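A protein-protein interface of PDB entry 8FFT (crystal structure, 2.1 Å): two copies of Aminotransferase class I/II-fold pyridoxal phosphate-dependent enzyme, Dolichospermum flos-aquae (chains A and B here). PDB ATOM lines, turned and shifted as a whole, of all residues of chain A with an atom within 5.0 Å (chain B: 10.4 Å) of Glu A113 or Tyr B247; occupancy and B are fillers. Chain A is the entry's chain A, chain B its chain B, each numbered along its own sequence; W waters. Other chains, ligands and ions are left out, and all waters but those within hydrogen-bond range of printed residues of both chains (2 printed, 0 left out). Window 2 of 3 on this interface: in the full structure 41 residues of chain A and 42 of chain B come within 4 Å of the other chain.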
ATOM      1  N   THR A  84       5.187  14.667  16.466  1.00  0.00           N
ATOM      2  CA  THR A  84       4.535  14.036  15.323  1.00  0.00           C
ATOM      3  C   THR A  84       5.240  12.745  14.921  1.00  0.00           C
ATOM      4  O   THR A  84       4.583  11.741  14.625  1.00  0.00           O
ATOM      5  CB  THR A  84       4.476  15.006  14.144  1.00  0.00           C
ATOM      6  OG1 THR A  84       3.652  16.125  14.488  1.00  0.00           O
ATOM      7  CG2 THR A  84       3.905  14.320  12.911  1.00  0.00           C
ATOM      8  N   LEU A  88       3.883   8.790  15.383  1.00  0.00           N
ATOM      9  CA  LEU A  88       3.899   7.814  14.300  1.00  0.00           C
ATOM     10  C   LEU A  88       4.619   6.533  14.707  1.00  0.00           C
ATOM     11  O   LEU A  88       4.098   5.429  14.507  1.00  0.00           O
ATOM     12  CB  LEU A  88       4.561   8.425  13.066  1.00  0.00           C
ATOM     13  CG  LEU A  88       4.784   7.437  11.931  1.00  0.00           C
ATOM     14  CD1 LEU A  88       3.441   7.006  11.368  1.00  0.00           C
ATOM     15  CD2 LEU A  88       5.672   8.047  10.853  1.00  0.00           C
ATOM     16  N   HIS A 109      -5.106  16.766  15.388  1.00  0.00           N
ATOM     17  CA  HIS A 109      -5.627  15.844  14.383  1.00  0.00           C
ATOM     18  C   HIS A 109      -4.728  14.628  14.171  1.00  0.00           C
ATOM     19  O   HIS A 109      -5.224  13.540  13.862  1.00  0.00           O
ATOM     20  CB  HIS A 109      -5.833  16.596  13.070  1.00  0.00           C
ATOM     21  CG  HIS A 109      -4.563  17.112  12.471  1.00  0.00           C
ATOM     22  ND1 HIS A 109      -3.966  16.532  11.372  1.00  0.00           N
ATOM     23  CD2 HIS A 109      -3.763  18.142  12.836  1.00  0.00           C
ATOM     24  CE1 HIS A 109      -2.861  17.193  11.075  1.00  0.00           C
ATOM     25  NE2 HIS A 109      -2.713  18.172  11.950  1.00  0.00           N
ATOM     26  N   VAL A 110      -3.412  14.787  14.327  1.00  0.00           N
ATOM     27  CA  VAL A 110      -2.490  13.671  14.127  1.00  0.00           C
ATOM     28  C   VAL A 110      -2.795  12.527  15.088  1.00  0.00           C
ATOM     29  O   VAL A 110      -2.594  11.351  14.755  1.00  0.00           O
ATOM     30  CB  VAL A 110      -1.037  14.174  14.259  1.00  0.00           C
ATOM     31  CG1 VAL A 110      -0.076  13.024  14.437  1.00  0.00           C
ATOM     32  CG2 VAL A 110      -0.656  15.002  13.041  1.00  0.00           C
ATOM     33  N   LEU A 111      -3.316  12.845  16.278  1.00  0.00           N
ATOM     34  CA  LEU A 111      -3.530  11.825  17.299  1.00  0.00           C
ATOM     35  C   LEU A 111      -4.585  10.801  16.892  1.00  0.00           C
ATOM     36  O   LEU A 111      -4.558   9.668  17.385  1.00  0.00           O
ATOM     37  CB  LEU A 111      -3.909  12.487  18.622  1.00  0.00           C
ATOM     38  CG  LEU A 111      -2.750  13.150  19.367  1.00  0.00           C
ATOM     39  CD1 LEU A 111      -3.267  13.962  20.547  1.00  0.00           C
ATOM     40  CD2 LEU A 111      -1.752  12.096  19.840  1.00  0.00           C
ATOM     41  N   TYR A 112      -5.522  11.162  16.014  1.00  0.00           N
ATOM     42  CA  TYR A 112      -6.457  10.176  15.490  1.00  0.00           C
ATOM     43  C   TYR A 112      -6.245   9.842  14.019  1.00  0.00           C
ATOM     44  O   TYR A 112      -6.675   8.769  13.587  1.00  0.00           O
ATOM     45  CB  TYR A 112      -7.913  10.623  15.704  1.00  0.00           C
ATOM     46  CG  TYR A 112      -8.287  11.988  15.174  1.00  0.00           C
ATOM     47  CD1 TYR A 112      -8.671  12.162  13.850  1.00  0.00           C
ATOM     48  CD2 TYR A 112      -8.277  13.097  16.006  1.00  0.00           C
ATOM     49  CE1 TYR A 112      -9.025  13.408  13.371  1.00  0.00           C
ATOM     50  CE2 TYR A 112      -8.632  14.339  15.540  1.00  0.00           C
ATOM     51  CZ  TYR A 112      -9.003  14.491  14.226  1.00  0.00           C
ATOM     52  OH  TYR A 112      -9.348  15.739  13.771  1.00  0.00           O
ATOM     53  N   GLU A 113      -5.604  10.717  13.245  1.00  0.00           N
ATOM     54  CA  GLU A 113      -5.395  10.438  11.823  1.00  0.00           C
ATOM     55  C   GLU A 113      -4.224   9.487  11.585  1.00  0.00           C
ATOM     56  O   GLU A 113      -4.313   8.592  10.736  1.00  0.00           O
ATOM     57  CB  GLU A 113      -5.196  11.754  11.071  1.00  0.00           C
ATOM     58  CG  GLU A 113      -6.508  12.439  10.753  1.00  0.00           C
ATOM     59  CD  GLU A 113      -6.340  13.854  10.245  1.00  0.00           C
ATOM     60  OE1 GLU A 113      -7.351  14.444   9.803  1.00  0.00           O
ATOM     61  OE2 GLU A 113      -5.206  14.376  10.287  1.00  0.00           O
ATOM     62  N   THR A 114      -3.128   9.647  12.323  1.00  0.00           N
ATOM     63  CA  THR A 114      -2.023   8.696  12.201  1.00  0.00           C
ATOM     64  C   THR A 114      -2.437   7.270  12.555  1.00  0.00           C
ATOM     65  O   THR A 114      -2.128   6.354  11.777  1.00  0.00           O
ATOM     66  CB  THR A 114      -0.838   9.168  13.052  1.00  0.00           C
ATOM     67  OG1 THR A 114      -0.267  10.348  12.472  1.00  0.00           O
ATOM     68  CG2 THR A 114       0.226   8.085  13.155  1.00  0.00           C
ATOM     69  N   PRO A 115      -3.142   7.003  13.665  1.00  0.00           N
ATOM     70  CA  PRO A 115      -3.612   5.623  13.890  1.00  0.00           C
ATOM     71  C   PRO A 115      -4.505   5.113  12.776  1.00  0.00           C
ATOM     72  O   PRO A 115      -4.388   3.948  12.368  1.00  0.00           O
ATOM     73  CB  PRO A 115      -4.380   5.727  15.215  1.00  0.00           C
ATOM     74  CG  PRO A 115      -3.820   6.906  15.884  1.00  0.00           C
ATOM     75  CD  PRO A 115      -3.463   7.874  14.810  1.00  0.00           C
ATOM     76  N   ALA A 116      -5.375   5.975  12.247  1.00  0.00           N
ATOM     77  CA  ALA A 116      -6.229   5.569  11.137  1.00  0.00           C
ATOM     78  C   ALA A 116      -5.399   5.185   9.919  1.00  0.00           C
ATOM     79  O   ALA A 116      -5.665   4.161   9.277  1.00  0.00           O
ATOM     80  CB  ALA A 116      -7.212   6.691  10.797  1.00  0.00           C
ATOM     81  N   PHE A 117      -4.375   5.985   9.593  1.00  0.00           N
ATOM     82  CA  PHE A 117      -3.494   5.646   8.475  1.00  0.00           C
ATOM     83  C   PHE A 117      -2.821   4.297   8.674  1.00  0.00           C
ATOM     84  O   PHE A 117      -2.584   3.569   7.702  1.00  0.00           O
ATOM     85  CB  PHE A 117      -2.413   6.718   8.290  1.00  0.00           C
ATOM     86  CG  PHE A 117      -2.904   7.980   7.646  1.00  0.00           C
ATOM     87  CD1 PHE A 117      -3.767   7.930   6.559  1.00  0.00           C
ATOM     88  CD2 PHE A 117      -2.473   9.218   8.096  1.00  0.00           C
ATOM     89  CE1 PHE A 117      -4.214   9.097   5.952  1.00  0.00           C
ATOM     90  CE2 PHE A 117      -2.915  10.390   7.487  1.00  0.00           C
ATOM     91  CZ  PHE A 117      -3.787  10.329   6.419  1.00  0.00           C
ATOM     92  N   THR B  55       6.842  24.548   4.574  1.00  0.00           N
ATOM     93  CA  THR B  55       6.568  23.115   4.628  1.00  0.00           C
ATOM     94  C   THR B  55       7.064  22.359   3.401  1.00  0.00           C
ATOM     95  O   THR B  55       7.091  21.125   3.435  1.00  0.00           O
ATOM     96  CB  THR B  55       5.069  22.860   4.818  1.00  0.00           C
ATOM     97  OG1 THR B  55       4.343  23.405   3.709  1.00  0.00           O
ATOM     98  CG2 THR B  55       4.572  23.498   6.110  1.00  0.00           C
ATOM     99  N   LEU B  78      10.408  18.732  -2.676  1.00  0.00           N
ATOM    100  CA  LEU B  78       9.931  18.684  -1.300  1.00  0.00           C
ATOM    101  C   LEU B  78      11.110  18.320  -0.410  1.00  0.00           C
ATOM    102  O   LEU B  78      11.678  17.233  -0.549  1.00  0.00           O
ATOM    103  CB  LEU B  78       8.790  17.676  -1.135  1.00  0.00           C
ATOM    104  CG  LEU B  78       8.202  17.507   0.271  1.00  0.00           C
ATOM    105  CD1 LEU B  78       7.471  18.772   0.742  1.00  0.00           C
ATOM    106  CD2 LEU B  78       7.273  16.295   0.341  1.00  0.00           C
ATOM    107  N   GLU B  85      13.125   9.902   5.386  1.00  0.00           N
ATOM    108  CA  GLU B  85      11.741  10.361   5.468  1.00  0.00           C
ATOM    109  C   GLU B  85      11.099  10.422   4.089  1.00  0.00           C
ATOM    110  O   GLU B  85       9.941  10.026   3.923  1.00  0.00           O
ATOM    111  CB  GLU B  85      11.660  11.728   6.145  1.00  0.00           C
ATOM    112  CG  GLU B  85      10.221  12.129   6.459  1.00  0.00           C
ATOM    113  CD  GLU B  85      10.082  13.566   6.924  1.00  0.00           C
ATOM    114  OE1 GLU B  85       9.201  13.828   7.776  1.00  0.00           O
ATOM    115  OE2 GLU B  85      10.856  14.432   6.454  1.00  0.00           O
ATOM    116  N   LEU B  88      10.082   6.959   3.088  1.00  0.00           N
ATOM    117  CA  LEU B  88       8.877   6.520   3.786  1.00  0.00           C
ATOM    118  C   LEU B  88       7.639   7.191   3.213  1.00  0.00           C
ATOM    119  O   LEU B  88       6.618   6.537   2.970  1.00  0.00           O
ATOM    120  CB  LEU B  88       8.991   6.812   5.280  1.00  0.00           C
ATOM    121  CG  LEU B  88       7.715   6.567   6.089  1.00  0.00           C
ATOM    122  CD1 LEU B  88       7.369   5.085   6.149  1.00  0.00           C
ATOM    123  CD2 LEU B  88       7.841   7.152   7.488  1.00  0.00           C
ATOM    124  N   ILE B  89       7.709   8.506   2.998  1.00  0.00           N
ATOM    125  CA  ILE B  89       6.553   9.238   2.492  1.00  0.00           C
ATOM    126  C   ILE B  89       6.183   8.754   1.099  1.00  0.00           C
ATOM    127  O   ILE B  89       5.012   8.498   0.803  1.00  0.00           O
ATOM    128  CB  ILE B  89       6.836  10.750   2.481  1.00  0.00           C
ATOM    129  CG1 ILE B  89       7.139  11.263   3.884  1.00  0.00           C
ATOM    130  CG2 ILE B  89       5.654  11.483   1.893  1.00  0.00           C
ATOM    131  CD1 ILE B  89       5.923  11.575   4.656  1.00  0.00           C
ATOM    132  N   LYS B  92       4.665   5.266   1.018  1.00  0.00           N
ATOM    133  CA  LYS B  92       3.333   5.303   1.615  1.00  0.00           C
ATOM    134  C   LYS B  92       2.294   5.821   0.628  1.00  0.00           C
ATOM    135  O   LYS B  92       1.254   5.186   0.418  1.00  0.00           O
ATOM    136  CB  LYS B  92       3.347   6.172   2.874  1.00  0.00           C
ATOM    137  CG  LYS B  92       2.040   6.163   3.655  1.00  0.00           C
ATOM    138  CD  LYS B  92       1.859   4.852   4.409  1.00  0.00           C
ATOM    139  CE  LYS B  92       0.742   4.945   5.436  1.00  0.00           C
ATOM    140  NZ  LYS B  92       0.434   3.608   6.026  1.00  0.00           N
ATOM    141  N   VAL B  93       2.564   6.965  -0.008  1.00  0.00           N
ATOM    142  CA  VAL B  93       1.570   7.561  -0.900  1.00  0.00           C
ATOM    143  C   VAL B  93       1.279   6.633  -2.076  1.00  0.00           C
ATOM    144  O   VAL B  93       0.136   6.530  -2.534  1.00  0.00           O
ATOM    145  CB  VAL B  93       2.004   8.968  -1.361  1.00  0.00           C
ATOM    146  CG1 VAL B  93       2.302   9.854  -0.161  1.00  0.00           C
ATOM    147  CG2 VAL B  93       3.190   8.910  -2.287  1.00  0.00           C
ATOM    148  N   LYS B 239       2.500  17.023  -4.177  1.00  0.00           N
ATOM    149  CA  LYS B 239       1.353  17.358  -3.345  1.00  0.00           C
ATOM    150  C   LYS B 239       0.989  16.207  -2.410  1.00  0.00           C
ATOM    151  O   LYS B 239       0.708  16.423  -1.226  1.00  0.00           O
ATOM    152  CB  LYS B 239       0.165  17.739  -4.229  1.00  0.00           C
ATOM    153  CG  LYS B 239      -0.995  18.312  -3.456  1.00  0.00           C
ATOM    154  CD  LYS B 239      -0.570  19.599  -2.753  1.00  0.00           C
ATOM    155  CE  LYS B 239      -1.083  19.668  -1.316  1.00  0.00           C
ATOM    156  NZ  LYS B 239      -0.353  18.742  -0.394  1.00  0.00           N
ATOM    157  N   ALA B 240       1.008  14.973  -2.920  1.00  0.00           N
ATOM    158  CA  ALA B 240       0.670  13.823  -2.089  1.00  0.00           C
ATOM    159  C   ALA B 240       1.713  13.599  -0.999  1.00  0.00           C
ATOM    160  O   ALA B 240       1.365  13.287   0.148  1.00  0.00           O
ATOM    161  CB  ALA B 240       0.523  12.575  -2.959  1.00  0.00           C
ATOM    162  N   CYS B 241       2.994  13.756  -1.337  1.00  0.00           N
ATOM    163  CA  CYS B 241       4.043  13.598  -0.338  1.00  0.00           C
ATOM    164  C   CYS B 241       4.012  14.726   0.681  1.00  0.00           C
ATOM    165  O   CYS B 241       4.169  14.487   1.883  1.00  0.00           O
ATOM    166  CB  CYS B 241       5.412  13.521  -1.017  1.00  0.00           C
ATOM    167  SG  CYS B 241       5.723  11.965  -1.892  1.00  0.00           S
ATOM    168  N   HIS B 242       3.805  15.962   0.223  1.00  0.00           N
ATOM    169  CA  HIS B 242       3.701  17.084   1.148  1.00  0.00           C
ATOM    170  C   HIS B 242       2.559  16.881   2.131  1.00  0.00           C
ATOM    171  O   HIS B 242       2.698  17.164   3.329  1.00  0.00           O
ATOM    172  CB  HIS B 242       3.518  18.389   0.373  1.00  0.00           C
ATOM    173  CG  HIS B 242       3.223  19.571   1.241  1.00  0.00           C
ATOM    174  ND1 HIS B 242       1.938  19.997   1.504  1.00  0.00           N
ATOM    175  CD2 HIS B 242       4.043  20.398   1.932  1.00  0.00           C
ATOM    176  CE1 HIS B 242       1.982  21.051   2.300  1.00  0.00           C
ATOM    177  NE2 HIS B 242       3.247  21.313   2.576  1.00  0.00           N
ATOM    178  N   PHE B 243       1.420  16.387   1.644  1.00  0.00           N
ATOM    179  CA  PHE B 243       0.294  16.137   2.535  1.00  0.00           C
ATOM    180  C   PHE B 243       0.669  15.142   3.620  1.00  0.00           C
ATOM    181  O   PHE B 243       0.448  15.391   4.812  1.00  0.00           O
ATOM    182  CB  PHE B 243      -0.906  15.625   1.743  1.00  0.00           C
ATOM    183  CG  PHE B 243      -1.944  14.959   2.601  1.00  0.00           C
ATOM    184  CD1 PHE B 243      -2.845  15.713   3.329  1.00  0.00           C
ATOM    185  CD2 PHE B 243      -2.016  13.576   2.677  1.00  0.00           C
ATOM    186  CE1 PHE B 243      -3.800  15.101   4.118  1.00  0.00           C
ATOM    187  CE2 PHE B 243      -2.968  12.959   3.460  1.00  0.00           C
ATOM    188  CZ  PHE B 243      -3.861  13.722   4.183  1.00  0.00           C
ATOM    189  N   PHE B 244       1.250  14.004   3.231  1.00  0.00           N
ATOM    190  CA  PHE B 244       1.523  12.979   4.224  1.00  0.00           C
ATOM    191  C   PHE B 244       2.699  13.337   5.119  1.00  0.00           C
ATOM    192  O   PHE B 244       2.820  12.768   6.209  1.00  0.00           O
ATOM    193  CB  PHE B 244       1.764  11.615   3.574  1.00  0.00           C
ATOM    194  CG  PHE B 244       1.754  10.488   4.570  1.00  0.00           C
ATOM    195  CD1 PHE B 244       0.565  10.082   5.158  1.00  0.00           C
ATOM    196  CD2 PHE B 244       2.931   9.859   4.946  1.00  0.00           C
ATOM    197  CE1 PHE B 244       0.549   9.060   6.098  1.00  0.00           C
ATOM    198  CE2 PHE B 244       2.923   8.832   5.880  1.00  0.00           C
ATOM    199  CZ  PHE B 244       1.732   8.433   6.455  1.00  0.00           C
ATOM    200  N   LYS B 245       3.544  14.283   4.704  1.00  0.00           N
ATOM    201  CA  LYS B 245       4.636  14.704   5.573  1.00  0.00           C
ATOM    202  C   LYS B 245       4.126  15.323   6.867  1.00  0.00           C
ATOM    203  O   LYS B 245       4.854  15.329   7.863  1.00  0.00           O
ATOM    204  CB  LYS B 245       5.563  15.668   4.834  1.00  0.00           C
ATOM    205  CG  LYS B 245       6.866  15.966   5.568  1.00  0.00           C
ATOM    206  CD  LYS B 245       7.867  16.680   4.662  1.00  0.00           C
ATOM    207  CE  LYS B 245       7.345  18.035   4.213  1.00  0.00           C
ATOM    208  NZ  LYS B 245       7.082  18.943   5.365  1.00  0.00           N
ATOM    209  N   ASP B 246       2.886  15.818   6.878  1.00  0.00           N
ATOM    210  CA  ASP B 246       2.283  16.346   8.099  1.00  0.00           C
ATOM    211  C   ASP B 246       2.164  15.288   9.191  1.00  0.00           C
ATOM    212  O   ASP B 246       1.940  15.634  10.356  1.00  0.00           O
ATOM    213  CB  ASP B 246       0.900  16.924   7.779  1.00  0.00           C
ATOM    214  CG  ASP B 246       0.464  17.998   8.760  1.00  0.00           C
ATOM    215  OD1 ASP B 246       0.137  17.669   9.927  1.00  0.00           O
ATOM    216  OD2 ASP B 246       0.447  19.182   8.362  1.00  0.00           O
ATOM    217  N   TYR B 247       2.309  14.012   8.844  1.00  0.00           N
ATOM    218  CA  TYR B 247       2.163  12.915   9.787  1.00  0.00           C
ATOM    219  C   TYR B 247       3.479  12.213  10.082  1.00  0.00           C
ATOM    220  O   TYR B 247       3.486  11.222  10.822  1.00  0.00           O
ATOM    221  CB  TYR B 247       1.131  11.916   9.256  1.00  0.00           C
ATOM    222  CG  TYR B 247      -0.180  12.589   8.951  1.00  0.00           C
ATOM    223  CD1 TYR B 247      -1.109  12.811   9.956  1.00  0.00           C
ATOM    224  CD2 TYR B 247      -0.475  13.044   7.670  1.00  0.00           C
ATOM    225  CE1 TYR B 247      -2.302  13.439   9.695  1.00  0.00           C
ATOM    226  CE2 TYR B 247      -1.673  13.679   7.397  1.00  0.00           C
ATOM    227  CZ  TYR B 247      -2.583  13.876   8.421  1.00  0.00           C
ATOM    228  OH  TYR B 247      -3.783  14.500   8.183  1.00  0.00           O
ATOM    229  N   THR B 248       4.590  12.698   9.531  1.00  0.00           N
ATOM    230  CA  THR B 248       5.912  12.206   9.897  1.00  0.00           C
ATOM    231  C   THR B 248       6.653  13.252  10.723  1.00  0.00           C
ATOM    232  O   THR B 248       6.904  13.027  11.907  1.00  0.00           O
ATOM    233  CB  THR B 248       6.717  11.791   8.664  1.00  0.00           C
ATOM    234  OG1 THR B 248       6.844  12.899   7.759  1.00  0.00           O
ATOM    235  CG2 THR B 248       6.027  10.620   7.967  1.00  0.00           C
ATOM    236  N   THR B 249       7.001  14.399  10.140  1.00  0.00           N
ATOM    237  CA  THR B 249       7.707  15.441  10.876  1.00  0.00           C
ATOM    238  C   THR B 249       7.151  16.840  10.674  1.00  0.00           C
ATOM    239  O   THR B 249       7.671  17.779  11.285  1.00  0.00           O
ATOM    240  CB  THR B 249       9.194  15.462  10.494  1.00  0.00           C
ATOM    241  OG1 THR B 249       9.322  15.741   9.091  1.00  0.00           O
ATOM    242  CG2 THR B 249       9.851  14.138  10.819  1.00  0.00           C
ATOM    243  N   HIS B 250       6.114  17.004   9.854  1.00  0.00           N
ATOM    244  CA  HIS B 250       5.541  18.307   9.521  1.00  0.00           C
ATOM    245  C   HIS B 250       6.538  19.164   8.740  1.00  0.00           C
ATOM    246  O   HIS B 250       6.385  19.343   7.528  1.00  0.00           O
ATOM    247  CB  HIS B 250       5.071  19.036  10.787  1.00  0.00           C
ATOM    248  CG  HIS B 250       4.318  20.300  10.512  1.00  0.00           C
ATOM    249  ND1 HIS B 250       4.444  21.427  11.295  1.00  0.00           N
ATOM    250  CD2 HIS B 250       3.413  20.606   9.555  1.00  0.00           C
ATOM    251  CE1 HIS B 250       3.656  22.377  10.824  1.00  0.00           C
ATOM    252  NE2 HIS B 250       3.019  21.904   9.769  1.00  0.00           N
ATOM    253  N   THR B 251       7.556  19.705   9.409  1.00  0.00           N
ATOM    254  CA  THR B 251       8.540  20.554   8.748  1.00  0.00           C
ATOM    255  C   THR B 251       9.940  20.177   9.208  1.00  0.00           C
ATOM    256  O   THR B 251      10.122  19.537  10.245  1.00  0.00           O
ATOM    257  CB  THR B 251       8.315  22.048   9.042  1.00  0.00           C
ATOM    258  OG1 THR B 251       8.491  22.289  10.442  1.00  0.00           O
ATOM    259  CG2 THR B 251       6.923  22.488   8.636  1.00  0.00           C
HETATM  260  O   HOH W   1       2.205  17.605  12.514  1.00  0.00           O
HETATM  261  O   HOH W   2       2.209  10.940  13.230  1.00  0.00           O
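The side-chain hydroxyl (OH) of Tyr B247 is in hydrogen-bond range of the side-chain carboxylate (OE2) of Glu A113 (2.5 Å).
The backbone carbonyl oxygen (O) of Phe A117 sits at hydrogen-bond distance from the side-chain amino group (NZ) of Lys B92, 3.5 Å away.
OG1 of Thr A114 sits close to O of Val A110, at 3.4 Å.
The backbone carbonyl oxygen of Lys B245 is in hydrogen-bond range of the side-chain hydroxyl of Thr B248 (3.1 Å).
ND1 of His A109 is in hydrogen-bond range of OE2 of Glu A113, 2.7 Å away.
The side-chain hydroxyl of Thr B248 is in hydrogen-bond range of the side-chain carboxylate of Glu B85.
CG2 of Thr A84 touches C of Tyr B247, 3.6 Å away.
O of Thr B248 touches CG2 of Thr A84, 3.4 Å away.
Leu A88 touches Tyr B247 (CB to O, 3.7 Å).
Leu A88 touches Thr B248.
His A109 touches Asp B246.
Tyr B247 touches His A109 (OH to ND1, 3.8 Å).
Tyr B247 touches Val A110.
Thr A114 touches Tyr B247.
CD2 of Phe A117 touches CE1 of Phe B244 (3.6 Å).
Phe A117 touches Tyr B247 (CE2 to CE2, 3.5 Å).
Glu A113 touches one residue of chain B.
Tyr B247 touches seven residues of chain A.
His A109 touches two residues of chain B.
Of chain B, only Asp B246 (3.8 Å) and Tyr B247 (3.8 Å) come within 4 Å of Val A110.
No residue of chain B comes within 4 Å of Tyr A112.
Thr A114 touches just one residue of chain B: Tyr B247 (3.6 Å).
No residue of chain B comes within 4 Å of Pro A115.
No residue of chain B comes within 4 Å of Ala A116.
Of the printed residues of chain B, Thr A84 touches Asp B246 (3.5 Å), Tyr B247 (3.6 Å) and Thr B248 (3.4 Å).
Of the printed residues of chain A, Phe B244 touches Phe A117.
Ile B89 touches none of the printed residues of chain A.
The nearest printed residue of chain A that does not touch Tyr B247 is Leu A111 (6.7 Å).
The nearest printed residue of chain B that does not touch Thr A84 is Thr B249 (4.2 Å).
Of the 20 printed residues of chain B, 5 touch a printed residue of chain A.
Printed residues of chain B that touch a printed residue of chain A: Lys B92, Phe B244, Asp B246, Tyr B247 and Thr B248.
Hydrophobic or aromatic side chains of chain B within 4 Å of the printed part of chain A: Phe B244 and Tyr B247.
Hydrophobic or aromatic side chains of chain A within 4 Å of the printed part of chain B: Leu A88, His A109, Val A110 and Phe A117.
Among the printed residues, 14 pairs touch across the chains.
Position printed for both chains: 88.
Of the 14 pairs that touch across the chains among the printed residues, none has its exchanged pair printed and touching as well.
Water W2 lies within hydrogen-bond range of OG1 of Thr A114, O of Tyr B247, O of Thr A84 and N of Leu A88.
Water W1 bridges OG1 of Thr A84 and O of Asp B246.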
